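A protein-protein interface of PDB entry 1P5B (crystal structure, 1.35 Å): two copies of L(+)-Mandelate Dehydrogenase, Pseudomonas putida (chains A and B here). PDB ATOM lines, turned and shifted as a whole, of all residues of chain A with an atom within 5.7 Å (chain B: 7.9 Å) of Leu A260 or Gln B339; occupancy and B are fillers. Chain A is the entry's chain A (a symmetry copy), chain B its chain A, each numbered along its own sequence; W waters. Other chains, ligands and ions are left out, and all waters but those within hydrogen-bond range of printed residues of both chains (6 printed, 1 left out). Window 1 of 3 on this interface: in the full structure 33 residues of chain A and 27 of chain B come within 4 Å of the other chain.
The side-chain hydroxyl (OG) of Ser B291 sits at hydrogen-bond distance from the side-chain sulfur (SG) of Cys A262, 3.7 Å away.
N of Phe B49 is in hydrogen-bond range of O of Cys A262 (2.8 Å).
The backbone carbonyl oxygen (O) of Asp A261 lies within hydrogen-bond range of the guanidinium group (NH1) of Arg B48 (3.0 Å).
The backbone carbonyl oxygen (O) of Ala A263 lies within hydrogen-bond range of the guanidinium group (NH1) of Arg B48 (2.8 Å).
The side-chain amide oxygen (OE1) of Gln B339 lies close to the backbone carbonyl oxygen (O) of Gln A259, 2.9 Å away.
NE of Arg B60 is in salt-bridge range of OD1 of Asp B334 (2.8 Å).
The backbone carbonyl oxygen (O) of Gln B339 lies within hydrogen-bond range of the guanidinium group (NH1) of Arg B53, at 2.7 Å.
N of Gly A36 lies within hydrogen-bond range of OD1 of Asp A261 (2.7 Å).
The backbone NH (N) of Lys B52 lies within hydrogen-bond range of the backbone carbonyl oxygen (O) of Ile B340, at 2.9 Å.
The side-chain amide oxygen (OE1) of Gln A259 lies within hydrogen-bond range of the backbone NH (N) of Gly A163 (2.8 Å).
O of Val B57 is in hydrogen-bond range of NH1 of Arg B60.
Among the printed residues, pairs that only touch across the chains: Ala A160 with Val B57 (3.9 Å), Val A161 with Arg B60 (3.9 Å), Val A161 with Arg B335 (3.98 Å), Val A161 with Ala B338 (3.7 Å), Val A161 with Gln B339 (3.7 Å), Asn A162 with Arg B335 (3.7 Å), Gly A163 with Gln B339 (3.96 Å), Tyr A164 with Arg B335 (3.4 Å), Leu A260 with Phe B49 (3.8 Å), Leu A260 with Pro B51 (3.7 Å), Leu A260 with Gln B339 (3.4 Å), Leu A260 with Ile B340 (3.8 Å), Cys A262 with Arg B48 (3.1 Å) and Ala A263 with Phe B49 (3.7 Å).
Leu A260 touches just these residues of chain B: Phe B49 (3.8 Å), Pro B51 (3.7 Å), Gln B339 (3.4 Å) and Ile B340 (3.8 Å).
Gln B339 touches four residues of chain A.
Of the printed residues of chain B, Cys A262 touches Arg B48, Phe B49 and Ser B291.
Of the printed residues of chain A, Ser B291 touches Cys A262.
Of the printed residues of chain B, Gly A163 touches Gln B339 (3.96 Å).
Pro B343 touches none of the printed residues of chain A.
The nearest residue of chain B that does not touch Leu A260 is Thr B336 (4.5 Å).
The nearest printed residue of chain B that does not touch Ala A263 is Pro B51 (5.0 Å).
Along chain B the printed residues that touch a printed residue of chain A span positions 48 to 340.
Hydrophobic or aromatic side chains of chain A within 4 Å of the printed part of chain B: Ala A160, Val A161, Tyr A164 and Leu A260.
Among the printed residues, 19 pairs touch across the chains.
No position is printed for both chains.
Water W6 lies within hydrogen-bond range of O of Gln A259, N of Tyr A164 and OE1 of Gln B339.
Water W1 bridges the side-chain hydroxyl (OG) of Ser B291 and the side-chain sulfur (SG) of Cys A262.
Water W3 lies within hydrogen-bond range of the side-chain hydroxyl (OG) of Ser B291 (2.7 Å) and the side-chain sulfur (SG) of Cys A262 (3.5 Å).
Water W4 lies within hydrogen-bond range of O of Asn A162 (2.8 Å) and NE of Arg B335 (2.8 Å).
Water W2 lies within hydrogen-bond range of O of Ala A263 (2.9 Å), O of Gly A36 (3.1 Å), ND2 of Asn A254 (3.3 Å) and NH1 of Arg B48 (3.4 Å).
Water W5 lies within hydrogen-bond range of the backbone NH of Ala A160 (2.9 Å) and the guanidinium group of Arg B53 (3.4 Å).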
ATOM      1  N   ALA A  31     -25.341  33.988   7.917  1.00  0.00           N
ATOM      2  CA  ALA A  31     -24.127  33.489   8.541  1.00  0.00           C
ATOM      3  C   ALA A  31     -22.908  33.693   7.648  1.00  0.00           C
ATOM      4  O   ALA A  31     -22.988  33.604   6.422  1.00  0.00           O
ATOM      5  CB  ALA A  31     -24.282  32.013   8.864  1.00  0.00           C
ATOM      6  N   GLY A  36     -24.985  31.416   1.734  1.00  0.00           N
ATOM      7  CA  GLY A  36     -26.198  30.659   1.992  1.00  0.00           C
ATOM      8  C   GLY A  36     -27.464  31.388   1.599  1.00  0.00           C
ATOM      9  O   GLY A  36     -28.303  30.833   0.892  1.00  0.00           O
ATOM     10  N   ALA A 160     -28.638  24.703  17.772  1.00  0.00           N
ATOM     11  CA  ALA A 160     -27.991  24.003  18.884  1.00  0.00           C
ATOM     12  C   ALA A 160     -26.938  24.936  19.470  1.00  0.00           C
ATOM     13  O   ALA A 160     -26.665  24.918  20.671  1.00  0.00           O
ATOM     14  CB  ALA A 160     -27.346  22.713  18.392  1.00  0.00           C
ATOM     15  N   VAL A 161     -26.338  25.736  18.593  1.00  0.00           N
ATOM     16  CA  VAL A 161     -25.361  26.751  18.965  1.00  0.00           C
ATOM     17  C   VAL A 161     -25.732  27.947  18.095  1.00  0.00           C
ATOM     18  O   VAL A 161     -26.407  27.789  17.076  1.00  0.00           O
ATOM     19  CB  VAL A 161     -23.894  26.327  18.681  1.00  0.00           C
ATOM     20  CG1 VAL A 161     -23.513  25.150  19.567  1.00  0.00           C
ATOM     21  CG2 VAL A 161     -23.711  25.989  17.212  1.00  0.00           C
ATOM     22  N   ASN A 162     -25.310  29.138  18.494  1.00  0.00           N
ATOM     23  CA  ASN A 162     -25.644  30.342  17.744  1.00  0.00           C
ATOM     24  C   ASN A 162     -24.886  30.481  16.428  1.00  0.00           C
ATOM     25  O   ASN A 162     -23.698  30.169  16.343  1.00  0.00           O
ATOM     26  CB  ASN A 162     -25.391  31.573  18.617  1.00  0.00           C
ATOM     27  CG  ASN A 162     -26.280  31.607  19.847  1.00  0.00           C
ATOM     28  OD1 ASN A 162     -25.994  32.311  20.815  1.00  0.00           O
ATOM     29  ND2 ASN A 162     -27.370  30.849  19.811  1.00  0.00           N
ATOM     30  N   GLY A 163     -25.588  30.953  15.404  1.00  0.00           N
ATOM     31  CA  GLY A 163     -24.964  31.151  14.109  1.00  0.00           C
ATOM     32  C   GLY A 163     -23.964  32.289  14.172  1.00  0.00           C
ATOM     33  O   GLY A 163     -24.109  33.216  14.971  1.00  0.00           O
ATOM     34  N   TYR A 164     -22.944  32.222  13.327  1.00  0.00           N
ATOM     35  CA  TYR A 164     -21.913  33.250  13.301  1.00  0.00           C
ATOM     36  C   TYR A 164     -22.292  34.313  12.275  1.00  0.00           C
ATOM     37  O   TYR A 164     -21.842  34.276  11.130  1.00  0.00           O
ATOM     38  CB  TYR A 164     -20.567  32.617  12.938  1.00  0.00           C
ATOM     39  CG  TYR A 164     -19.359  33.412  13.382  1.00  0.00           C
ATOM     40  CD1 TYR A 164     -19.052  33.554  14.735  1.00  0.00           C
ATOM     41  CD2 TYR A 164     -18.507  33.999  12.448  1.00  0.00           C
ATOM     42  CE1 TYR A 164     -17.925  34.256  15.148  1.00  0.00           C
ATOM     43  CE2 TYR A 164     -17.375  34.706  12.851  1.00  0.00           C
ATOM     44  CZ  TYR A 164     -17.090  34.828  14.203  1.00  0.00           C
ATOM     45  OH  TYR A 164     -15.961  35.505  14.611  1.00  0.00           O
ATOM     46  N   ASN A 254     -33.294  25.980   6.461  1.00  0.00           N
ATOM     47  CA  ASN A 254     -31.927  26.237   6.896  1.00  0.00           C
ATOM     48  C   ASN A 254     -31.915  27.547   7.683  1.00  0.00           C
ATOM     49  O   ASN A 254     -30.899  28.235   7.789  1.00  0.00           O
ATOM     50  CB  ASN A 254     -30.882  26.236   5.755  1.00  0.00           C
ATOM     51  CG  ASN A 254     -31.145  27.259   4.664  1.00  0.00           C
ATOM     52  OD1 ASN A 254     -31.642  28.358   4.905  1.00  0.00           O
ATOM     53  ND2 ASN A 254     -30.762  26.900   3.440  1.00  0.00           N
ATOM     54  N   GLY A 257     -30.718  30.924   6.017  1.00  0.00           N
ATOM     55  CA  GLY A 257     -29.292  31.149   5.842  1.00  0.00           C
ATOM     56  C   GLY A 257     -28.621  31.861   7.001  1.00  0.00           C
ATOM     57  O   GLY A 257     -27.512  32.374   6.866  1.00  0.00           O
ATOM     58  N   ARG A 258     -29.278  31.865   8.157  1.00  0.00           N
ATOM     59  CA  ARG A 258     -28.762  32.559   9.331  1.00  0.00           C
ATOM     60  C   ARG A 258     -27.930  31.725  10.291  1.00  0.00           C
ATOM     61  O   ARG A 258     -27.343  32.270  11.229  1.00  0.00           O
ATOM     62  CB  ARG A 258     -29.928  33.179  10.105  1.00  0.00           C
ATOM     63  CG  ARG A 258     -30.734  34.174   9.297  1.00  0.00           C
ATOM     64  CD  ARG A 258     -32.052  34.499   9.975  1.00  0.00           C
ATOM     65  NE  ARG A 258     -31.913  35.221  11.239  1.00  0.00           N
ATOM     66  CZ  ARG A 258     -31.671  36.525  11.335  1.00  0.00           C
ATOM     67  NH1 ARG A 258     -31.533  37.262  10.240  1.00  0.00           N
ATOM     68  NH2 ARG A 258     -31.597  37.099  12.529  1.00  0.00           N
ATOM     69  N   GLN A 259     -27.863  30.421  10.061  1.00  0.00           N
ATOM     70  CA  GLN A 259     -27.126  29.554  10.969  1.00  0.00           C
ATOM     71  C   GLN A 259     -25.865  28.901  10.419  1.00  0.00           C
ATOM     72  O   GLN A 259     -24.814  28.959  11.052  1.00  0.00           O
ATOM     73  CB  GLN A 259     -28.063  28.476  11.524  1.00  0.00           C
ATOM     74  CG  GLN A 259     -29.213  29.020  12.382  1.00  0.00           C
ATOM     75  CD  GLN A 259     -28.742  29.920  13.519  1.00  0.00           C
ATOM     76  OE1 GLN A 259     -27.754  29.632  14.184  1.00  0.00           O
ATOM     77  NE2 GLN A 259     -29.466  31.010  13.752  1.00  0.00           N
ATOM     78  N   LEU A 260     -25.966  28.277   9.253  1.00  0.00           N
ATOM     79  CA  LEU A 260     -24.827  27.591   8.647  1.00  0.00           C
ATOM     80  C   LEU A 260     -24.755  28.037   7.194  1.00  0.00           C
ATOM     81  O   LEU A 260     -25.572  27.629   6.370  1.00  0.00           O
ATOM     82  CB  LEU A 260     -25.040  26.081   8.739  1.00  0.00           C
ATOM     83  CG  LEU A 260     -23.955  25.155   8.191  1.00  0.00           C
ATOM     84  CD1 LEU A 260     -22.642  25.368   8.941  1.00  0.00           C
ATOM     85  CD2 LEU A 260     -24.426  23.717   8.341  1.00  0.00           C
ATOM     86  N   ASP A 261     -23.772  28.870   6.879  1.00  0.00           N
ATOM     87  CA  ASP A 261     -23.650  29.419   5.535  1.00  0.00           C
ATOM     88  C   ASP A 261     -23.612  28.399   4.405  1.00  0.00           C
ATOM     89  O   ASP A 261     -24.203  28.626   3.349  1.00  0.00           O
ATOM     90  CB  ASP A 261     -22.422  30.330   5.454  1.00  0.00           C
ATOM     91  CG  ASP A 261     -22.524  31.337   4.322  1.00  0.00           C
ATOM     92  OD1 ASP A 261     -23.648  31.835   4.083  1.00  0.00           O
ATOM     93  OD2 ASP A 261     -21.493  31.648   3.685  1.00  0.00           O
ATOM     94  N   CYS A 262     -22.945  27.272   4.625  1.00  0.00           N
ATOM     95  CA  CYS A 262     -22.829  26.259   3.583  1.00  0.00           C
ATOM     96  C   CYS A 262     -23.894  25.174   3.601  1.00  0.00           C
ATOM     97  O   CYS A 262     -23.747  24.143   2.953  1.00  0.00           O
ATOM     98  CB  CYS A 262     -21.439  25.625   3.629  1.00  0.00           C
ATOM     99  SG  CYS A 262     -20.128  26.812   3.289  1.00  0.00           S
ATOM    100  N   ALA A 263     -24.969  25.404   4.345  1.00  0.00           N
ATOM    101  CA  ALA A 263     -26.059  24.437   4.386  1.00  0.00           C
ATOM    102  C   ALA A 263     -26.739  24.375   3.020  1.00  0.00           C
ATOM    103  O   ALA A 263     -26.775  25.367   2.287  1.00  0.00           O
ATOM    104  CB  ALA A 263     -27.083  24.844   5.445  1.00  0.00           C
ATOM    105  N   ARG B  48     -21.986  21.225  -0.117  1.00  0.00           N
ATOM    106  CA  ARG B  48     -22.769  21.927   0.887  1.00  0.00           C
ATOM    107  C   ARG B  48     -23.080  20.912   1.980  1.00  0.00           C
ATOM    108  O   ARG B  48     -22.922  19.708   1.777  1.00  0.00           O
ATOM    109  CB  ARG B  48     -24.038  22.543   0.287  1.00  0.00           C
ATOM    110  CG  ARG B  48     -23.729  23.887  -0.368  1.00  0.00           C
ATOM    111  CD  ARG B  48     -24.950  24.700  -0.791  1.00  0.00           C
ATOM    112  NE  ARG B  48     -24.531  26.057  -1.149  1.00  0.00           N
ATOM    113  CZ  ARG B  48     -24.519  27.101  -0.321  1.00  0.00           C
ATOM    114  NH1 ARG B  48     -24.921  26.984   0.943  1.00  0.00           N
ATOM    115  NH2 ARG B  48     -24.064  28.272  -0.749  1.00  0.00           N
ATOM    116  N   PHE B  49     -23.495  21.397   3.145  1.00  0.00           N
ATOM    117  CA  PHE B  49     -23.775  20.522   4.274  1.00  0.00           C
ATOM    118  C   PHE B  49     -25.208  20.054   4.401  1.00  0.00           C
ATOM    119  O   PHE B  49     -26.146  20.789   4.094  1.00  0.00           O
ATOM    120  CB  PHE B  49     -23.421  21.218   5.592  1.00  0.00           C
ATOM    121  CG  PHE B  49     -21.960  21.513   5.766  1.00  0.00           C
ATOM    122  CD1 PHE B  49     -21.019  20.489   5.742  1.00  0.00           C
ATOM    123  CD2 PHE B  49     -21.532  22.813   6.006  1.00  0.00           C
ATOM    124  CE1 PHE B  49     -19.667  20.760   5.958  1.00  0.00           C
ATOM    125  CE2 PHE B  49     -20.185  23.094   6.225  1.00  0.00           C
ATOM    126  CZ  PHE B  49     -19.253  22.065   6.201  1.00  0.00           C
ATOM    127  N   LYS B  50     -25.351  18.823   4.878  1.00  0.00           N
ATOM    128  CA  LYS B  50     -26.644  18.220   5.161  1.00  0.00           C
ATOM    129  C   LYS B  50     -26.526  17.815   6.628  1.00  0.00           C
ATOM    130  O   LYS B  50     -26.122  16.700   6.960  1.00  0.00           O
ATOM    131  CB  LYS B  50     -26.905  17.002   4.271  1.00  0.00           C
ATOM    132  CG  LYS B  50     -27.133  17.377   2.817  1.00  0.00           C
ATOM    133  CD  LYS B  50     -27.509  16.175   1.964  1.00  0.00           C
ATOM    134  CE  LYS B  50     -28.861  15.608   2.365  1.00  0.00           C
ATOM    135  NZ  LYS B  50     -29.331  14.594   1.376  1.00  0.00           N
ATOM    136  N   PRO B  51     -26.832  18.754   7.530  1.00  0.00           N
ATOM    137  CA  PRO B  51     -26.767  18.519   8.972  1.00  0.00           C
ATOM    138  C   PRO B  51     -27.638  17.369   9.441  1.00  0.00           C
ATOM    139  O   PRO B  51     -28.660  17.050   8.828  1.00  0.00           O
ATOM    140  CB  PRO B  51     -27.247  19.841   9.560  1.00  0.00           C
ATOM    141  CG  PRO B  51     -26.791  20.845   8.550  1.00  0.00           C
ATOM    142  CD  PRO B  51     -27.127  20.170   7.242  1.00  0.00           C
ATOM    143  N   LYS B  52     -27.206  16.743  10.529  1.00  0.00           N
ATOM    144  CA  LYS B  52     -27.953  15.666  11.159  1.00  0.00           C
ATOM    145  C   LYS B  52     -28.514  16.332  12.409  1.00  0.00           C
ATOM    146  O   LYS B  52     -27.762  16.748  13.294  1.00  0.00           O
ATOM    147  CB  LYS B  52     -27.028  14.506  11.522  1.00  0.00           C
ATOM    148  CG  LYS B  52     -26.401  13.847  10.303  1.00  0.00           C
ATOM    149  CD  LYS B  52     -25.603  12.612  10.670  1.00  0.00           C
ATOM    150  CE  LYS B  52     -24.905  12.035   9.447  1.00  0.00           C
ATOM    151  NZ  LYS B  52     -25.863  11.729   8.351  1.00  0.00           N
ATOM    152  N   ARG B  53     -29.836  16.457  12.460  1.00  0.00           N
ATOM    153  CA  ARG B  53     -30.509  17.114  13.573  1.00  0.00           C
ATOM    154  C   ARG B  53     -30.804  16.201  14.750  1.00  0.00           C
ATOM    155  O   ARG B  53     -30.756  14.980  14.635  1.00  0.00           O
ATOM    156  CB  ARG B  53     -31.817  17.747  13.091  1.00  0.00           C
ATOM    157  CG  ARG B  53     -31.634  18.855  12.066  1.00  0.00           C
ATOM    158  CD  ARG B  53     -30.915  20.050  12.661  1.00  0.00           C
ATOM    159  NE  ARG B  53     -30.647  21.065  11.650  1.00  0.00           N
ATOM    160  CZ  ARG B  53     -29.512  21.750  11.565  1.00  0.00           C
ATOM    161  NH1 ARG B  53     -28.534  21.535  12.434  1.00  0.00           N
ATOM    162  NH2 ARG B  53     -29.349  22.637  10.595  1.00  0.00           N
ATOM    163  N   VAL B  57     -25.070  17.387  20.870  1.00  0.00           N
ATOM    164  CA  VAL B  57     -23.778  17.999  20.583  1.00  0.00           C
ATOM    165  C   VAL B  57     -23.340  18.895  21.738  1.00  0.00           C
ATOM    166  O   VAL B  57     -22.600  19.857  21.548  1.00  0.00           O
ATOM    167  CB  VAL B  57     -23.811  18.825  19.261  1.00  0.00           C
ATOM    168  CG1 VAL B  57     -24.076  17.901  18.082  1.00  0.00           C
ATOM    169  CG2 VAL B  57     -24.872  19.908  19.332  1.00  0.00           C
ATOM    170  N   ARG B  60     -18.487  18.281  22.640  1.00  0.00           N
ATOM    171  CA  ARG B  60     -17.807  18.117  21.366  1.00  0.00           C
ATOM    172  C   ARG B  60     -16.302  17.949  21.527  1.00  0.00           C
ATOM    173  O   ARG B  60     -15.712  18.430  22.495  1.00  0.00           O
ATOM    174  CB  ARG B  60     -18.123  19.316  20.472  1.00  0.00           C
ATOM    175  CG  ARG B  60     -19.622  19.561  20.324  1.00  0.00           C
ATOM    176  CD  ARG B  60     -19.920  20.703  19.374  1.00  0.00           C
ATOM    177  NE  ARG B  60     -19.503  22.004  19.891  1.00  0.00           N
ATOM    178  CZ  ARG B  60     -20.216  22.743  20.735  1.00  0.00           C
ATOM    179  NH1 ARG B  60     -21.395  22.316  21.172  1.00  0.00           N
ATOM    180  NH2 ARG B  60     -19.760  23.926  21.125  1.00  0.00           N
ATOM    181  N   SER B 291     -15.566  25.832   7.537  1.00  0.00           N
ATOM    182  CA  SER B 291     -16.358  24.968   6.669  1.00  0.00           C
ATOM    183  C   SER B 291     -15.493  24.316   5.590  1.00  0.00           C
ATOM    184  O   SER B 291     -15.742  23.173   5.215  1.00  0.00           O
ATOM    185  CB  SER B 291     -17.513  25.751   6.037  1.00  0.00           C
ATOM    186  OG  SER B 291     -17.049  26.860   5.294  1.00  0.00           O
ATOM    187  N   ALA B 331     -12.792  27.739  16.963  1.00  0.00           N
ATOM    188  CA  ALA B 331     -14.171  28.017  17.350  1.00  0.00           C
ATOM    189  C   ALA B 331     -15.090  27.811  16.147  1.00  0.00           C
ATOM    190  O   ALA B 331     -16.244  27.410  16.290  1.00  0.00           O
ATOM    191  CB  ALA B 331     -14.292  29.442  17.864  1.00  0.00           C
ATOM    192  N   ASP B 332     -14.555  28.091  14.964  1.00  0.00           N
ATOM    193  CA  ASP B 332     -15.267  27.950  13.700  1.00  0.00           C
ATOM    194  C   ASP B 332     -15.548  26.466  13.436  1.00  0.00           C
ATOM    195  O   ASP B 332     -16.679  26.073  13.148  1.00  0.00           O
ATOM    196  CB  ASP B 332     -14.390  28.540  12.592  1.00  0.00           C
ATOM    197  CG  ASP B 332     -15.089  28.622  11.253  1.00  0.00           C
ATOM    198  OD1 ASP B 332     -16.134  27.967  11.064  1.00  0.00           O
ATOM    199  OD2 ASP B 332     -14.565  29.344  10.379  1.00  0.00           O
ATOM    200  N   ILE B 333     -14.508  25.646  13.535  1.00  0.00           N
ATOM    201  CA  ILE B 333     -14.643  24.210  13.325  1.00  0.00           C
ATOM    202  C   ILE B 333     -15.609  23.623  14.352  1.00  0.00           C
ATOM    203  O   ILE B 333     -16.488  22.834  14.008  1.00  0.00           O
ATOM    204  CB  ILE B 333     -13.271  23.513  13.451  1.00  0.00           C
ATOM    205  CG1 ILE B 333     -12.362  23.957  12.301  1.00  0.00           C
ATOM    206  CG2 ILE B 333     -13.440  22.001  13.465  1.00  0.00           C
ATOM    207  CD1 ILE B 333     -10.921  23.514  12.463  1.00  0.00           C
ATOM    208  N   ASP B 334     -15.440  24.019  15.612  1.00  0.00           N
ATOM    209  CA  ASP B 334     -16.294  23.544  16.696  1.00  0.00           C
ATOM    210  C   ASP B 334     -17.757  23.888  16.422  1.00  0.00           C
ATOM    211  O   ASP B 334     -18.648  23.041  16.540  1.00  0.00           O
ATOM    212  CB  ASP B 334     -15.856  24.184  18.014  1.00  0.00           C
ATOM    213  CG  ASP B 334     -16.776  23.830  19.161  1.00  0.00           C
ATOM    214  OD1 ASP B 334     -16.832  22.639  19.527  1.00  0.00           O
ATOM    215  OD2 ASP B 334     -17.444  24.742  19.688  1.00  0.00           O
ATOM    216  N   ARG B 335     -17.997  25.140  16.055  1.00  0.00           N
ATOM    217  CA  ARG B 335     -19.339  25.617  15.752  1.00  0.00           C
ATOM    218  C   ARG B 335     -19.945  24.813  14.603  1.00  0.00           C
ATOM    219  O   ARG B 335     -21.108  24.406  14.655  1.00  0.00           O
ATOM    220  CB  ARG B 335     -19.273  27.099  15.381  1.00  0.00           C
ATOM    221  CG  ARG B 335     -20.608  27.771  15.152  1.00  0.00           C
ATOM    222  CD  ARG B 335     -20.409  29.255  14.862  1.00  0.00           C
ATOM    223  NE  ARG B 335     -19.692  29.936  15.940  1.00  0.00           N
ATOM    224  CZ  ARG B 335     -18.451  30.411  15.849  1.00  0.00           C
ATOM    225  NH1 ARG B 335     -17.760  30.294  14.724  1.00  0.00           N
ATOM    226  NH2 ARG B 335     -17.892  31.005  16.895  1.00  0.00           N
ATOM    227  N   THR B 336     -19.145  24.582  13.568  1.00  0.00           N
ATOM    228  CA  THR B 336     -19.596  23.833  12.405  1.00  0.00           C
ATOM    229  C   THR B 336     -19.965  22.399  12.777  1.00  0.00           C
ATOM    230  O   THR B 336     -20.979  21.875  12.317  1.00  0.00           O
ATOM    231  CB  THR B 336     -18.508  23.826  11.314  1.00  0.00           C
ATOM    232  OG1 THR B 336     -18.207  25.177  10.944  1.00  0.00           O
ATOM    233  CG2 THR B 336     -18.983  23.066  10.080  1.00  0.00           C
ATOM    234  N   LEU B 337     -19.143  21.760  13.604  1.00  0.00           N
ATOM    235  CA  LEU B 337     -19.423  20.391  14.028  1.00  0.00           C
ATOM    236  C   LEU B 337     -20.757  20.318  14.758  1.00  0.00           C
ATOM    237  O   LEU B 337     -21.546  19.396  14.542  1.00  0.00           O
ATOM    238  CB  LEU B 337     -18.318  19.874  14.954  1.00  0.00           C
ATOM    239  CG  LEU B 337     -16.948  19.643  14.312  1.00  0.00           C
ATOM    240  CD1 LEU B 337     -15.979  19.116  15.360  1.00  0.00           C
ATOM    241  CD2 LEU B 337     -17.079  18.658  13.161  1.00  0.00           C
ATOM    242  N   ALA B 338     -21.004  21.290  15.628  1.00  0.00           N
ATOM    243  CA  ALA B 338     -22.247  21.324  16.383  1.00  0.00           C
ATOM    244  C   ALA B 338     -23.420  21.483  15.428  1.00  0.00           C
ATOM    245  O   ALA B 338     -24.421  20.773  15.531  1.00  0.00           O
ATOM    246  CB  ALA B 338     -22.226  22.479  17.376  1.00  0.00           C
ATOM    247  N   GLN B 339     -23.275  22.407  14.484  1.00  0.00           N
ATOM    248  CA  GLN B 339     -24.327  22.692  13.520  1.00  0.00           C
ATOM    249  C   GLN B 339     -24.657  21.554  12.565  1.00  0.00           C
ATOM    250  O   GLN B 339     -25.805  21.426  12.142  1.00  0.00           O
ATOM    251  CB  GLN B 339     -23.968  23.954  12.736  1.00  0.00           C
ATOM    252  CG  GLN B 339     -24.039  25.217  13.586  1.00  0.00           C
ATOM    253  CD  GLN B 339     -23.269  26.378  12.990  1.00  0.00           C
ATOM    254  OE1 GLN B 339     -23.580  27.540  13.249  1.00  0.00           O
ATOM    255  NE2 GLN B 339     -22.245  26.067  12.203  1.00  0.00           N
ATOM    256  N   ILE B 340     -23.679  20.724  12.217  1.00  0.00           N
ATOM    257  CA  ILE B 340     -23.969  19.618  11.307  1.00  0.00           C
ATOM    258  C   ILE B 340     -24.277  18.319  12.050  1.00  0.00           C
ATOM    259  O   ILE B 340     -24.540  17.290  11.434  1.00  0.00           O
ATOM    260  CB  ILE B 340     -22.824  19.378  10.278  1.00  0.00           C
ATOM    261  CG1 ILE B 340     -21.553  18.890  10.978  1.00  0.00           C
ATOM    262  CG2 ILE B 340     -22.559  20.665   9.498  1.00  0.00           C
ATOM    263  CD1 ILE B 340     -20.435  18.515  10.010  1.00  0.00           C
ATOM    264  N   GLY B 341     -24.244  18.378  13.379  1.00  0.00           N
ATOM    265  CA  GLY B 341     -24.556  17.206  14.181  1.00  0.00           C
ATOM    266  C   GLY B 341     -23.485  16.139  14.276  1.00  0.00           C
ATOM    267  O   GLY B 341     -23.796  14.951  14.367  1.00  0.00           O
ATOM    268  N   CYS B 342     -22.223  16.552  14.249  1.00  0.00           N
ATOM    269  CA  CYS B 342     -21.113  15.612  14.354  1.00  0.00           C
ATOM    270  C   CYS B 342     -20.217  16.098  15.492  1.00  0.00           C
ATOM    271  O   CYS B 342     -19.189  16.736  15.261  1.00  0.00           O
ATOM    272  CB  CYS B 342     -20.334  15.568  13.037  1.00  0.00           C
ATOM    273  SG  CYS B 342     -19.160  14.209  12.921  1.00  0.00           S
ATOM    274  N   PRO B 343     -20.598  15.790  16.743  1.00  0.00           N
ATOM    275  CA  PRO B 343     -19.850  16.202  17.937  1.00  0.00           C
ATOM    276  C   PRO B 343     -18.386  15.796  18.023  1.00  0.00           C
ATOM    277  O   PRO B 343     -17.570  16.546  18.561  1.00  0.00           O
ATOM    278  CB  PRO B 343     -20.694  15.641  19.083  1.00  0.00           C
ATOM    279  CG  PRO B 343     -21.310  14.427  18.490  1.00  0.00           C
ATOM    280  CD  PRO B 343     -21.716  14.902  17.109  1.00  0.00           C
ATOM    281  N   TYR B 352     -22.317  13.807   5.506  1.00  0.00           N
ATOM    282  CA  TYR B 352     -22.699  15.147   5.938  1.00  0.00           C
ATOM    283  C   TYR B 352     -22.627  16.139   4.789  1.00  0.00           C
ATOM    284  O   TYR B 352     -22.920  17.319   4.970  1.00  0.00           O
ATOM    285  CB  TYR B 352     -21.779  15.648   7.053  1.00  0.00           C
ATOM    286  CG  TYR B 352     -21.881  14.876   8.343  1.00  0.00           C
ATOM    287  CD1 TYR B 352     -21.158  13.698   8.534  1.00  0.00           C
ATOM    288  CD2 TYR B 352     -22.708  15.321   9.374  1.00  0.00           C
ATOM    289  CE1 TYR B 352     -21.257  12.980   9.724  1.00  0.00           C
ATOM    290  CE2 TYR B 352     -22.814  14.613  10.564  1.00  0.00           C
ATOM    291  CZ  TYR B 352     -22.088  13.446  10.733  1.00  0.00           C
ATOM    292  OH  TYR B 352     -22.209  12.749  11.910  1.00  0.00           O
HETATM  293  O   HOH W   1     -18.756  28.912   5.866  1.00  0.00           O
HETATM  294  O   HOH W   2     -27.979  28.001   2.165  1.00  0.00           O
HETATM  295  O   HOH W   3     -16.708  26.140   2.676  1.00  0.00           O
HETATM  296  O   HOH W   4     -21.559  29.675  18.013  1.00  0.00           O
HETATM  297  O   HOH W   5     -27.968  23.442  15.228  1.00  0.00           O
HETATM  298  O   HOH W   6     -22.528  29.996  11.653  1.00  0.00           O
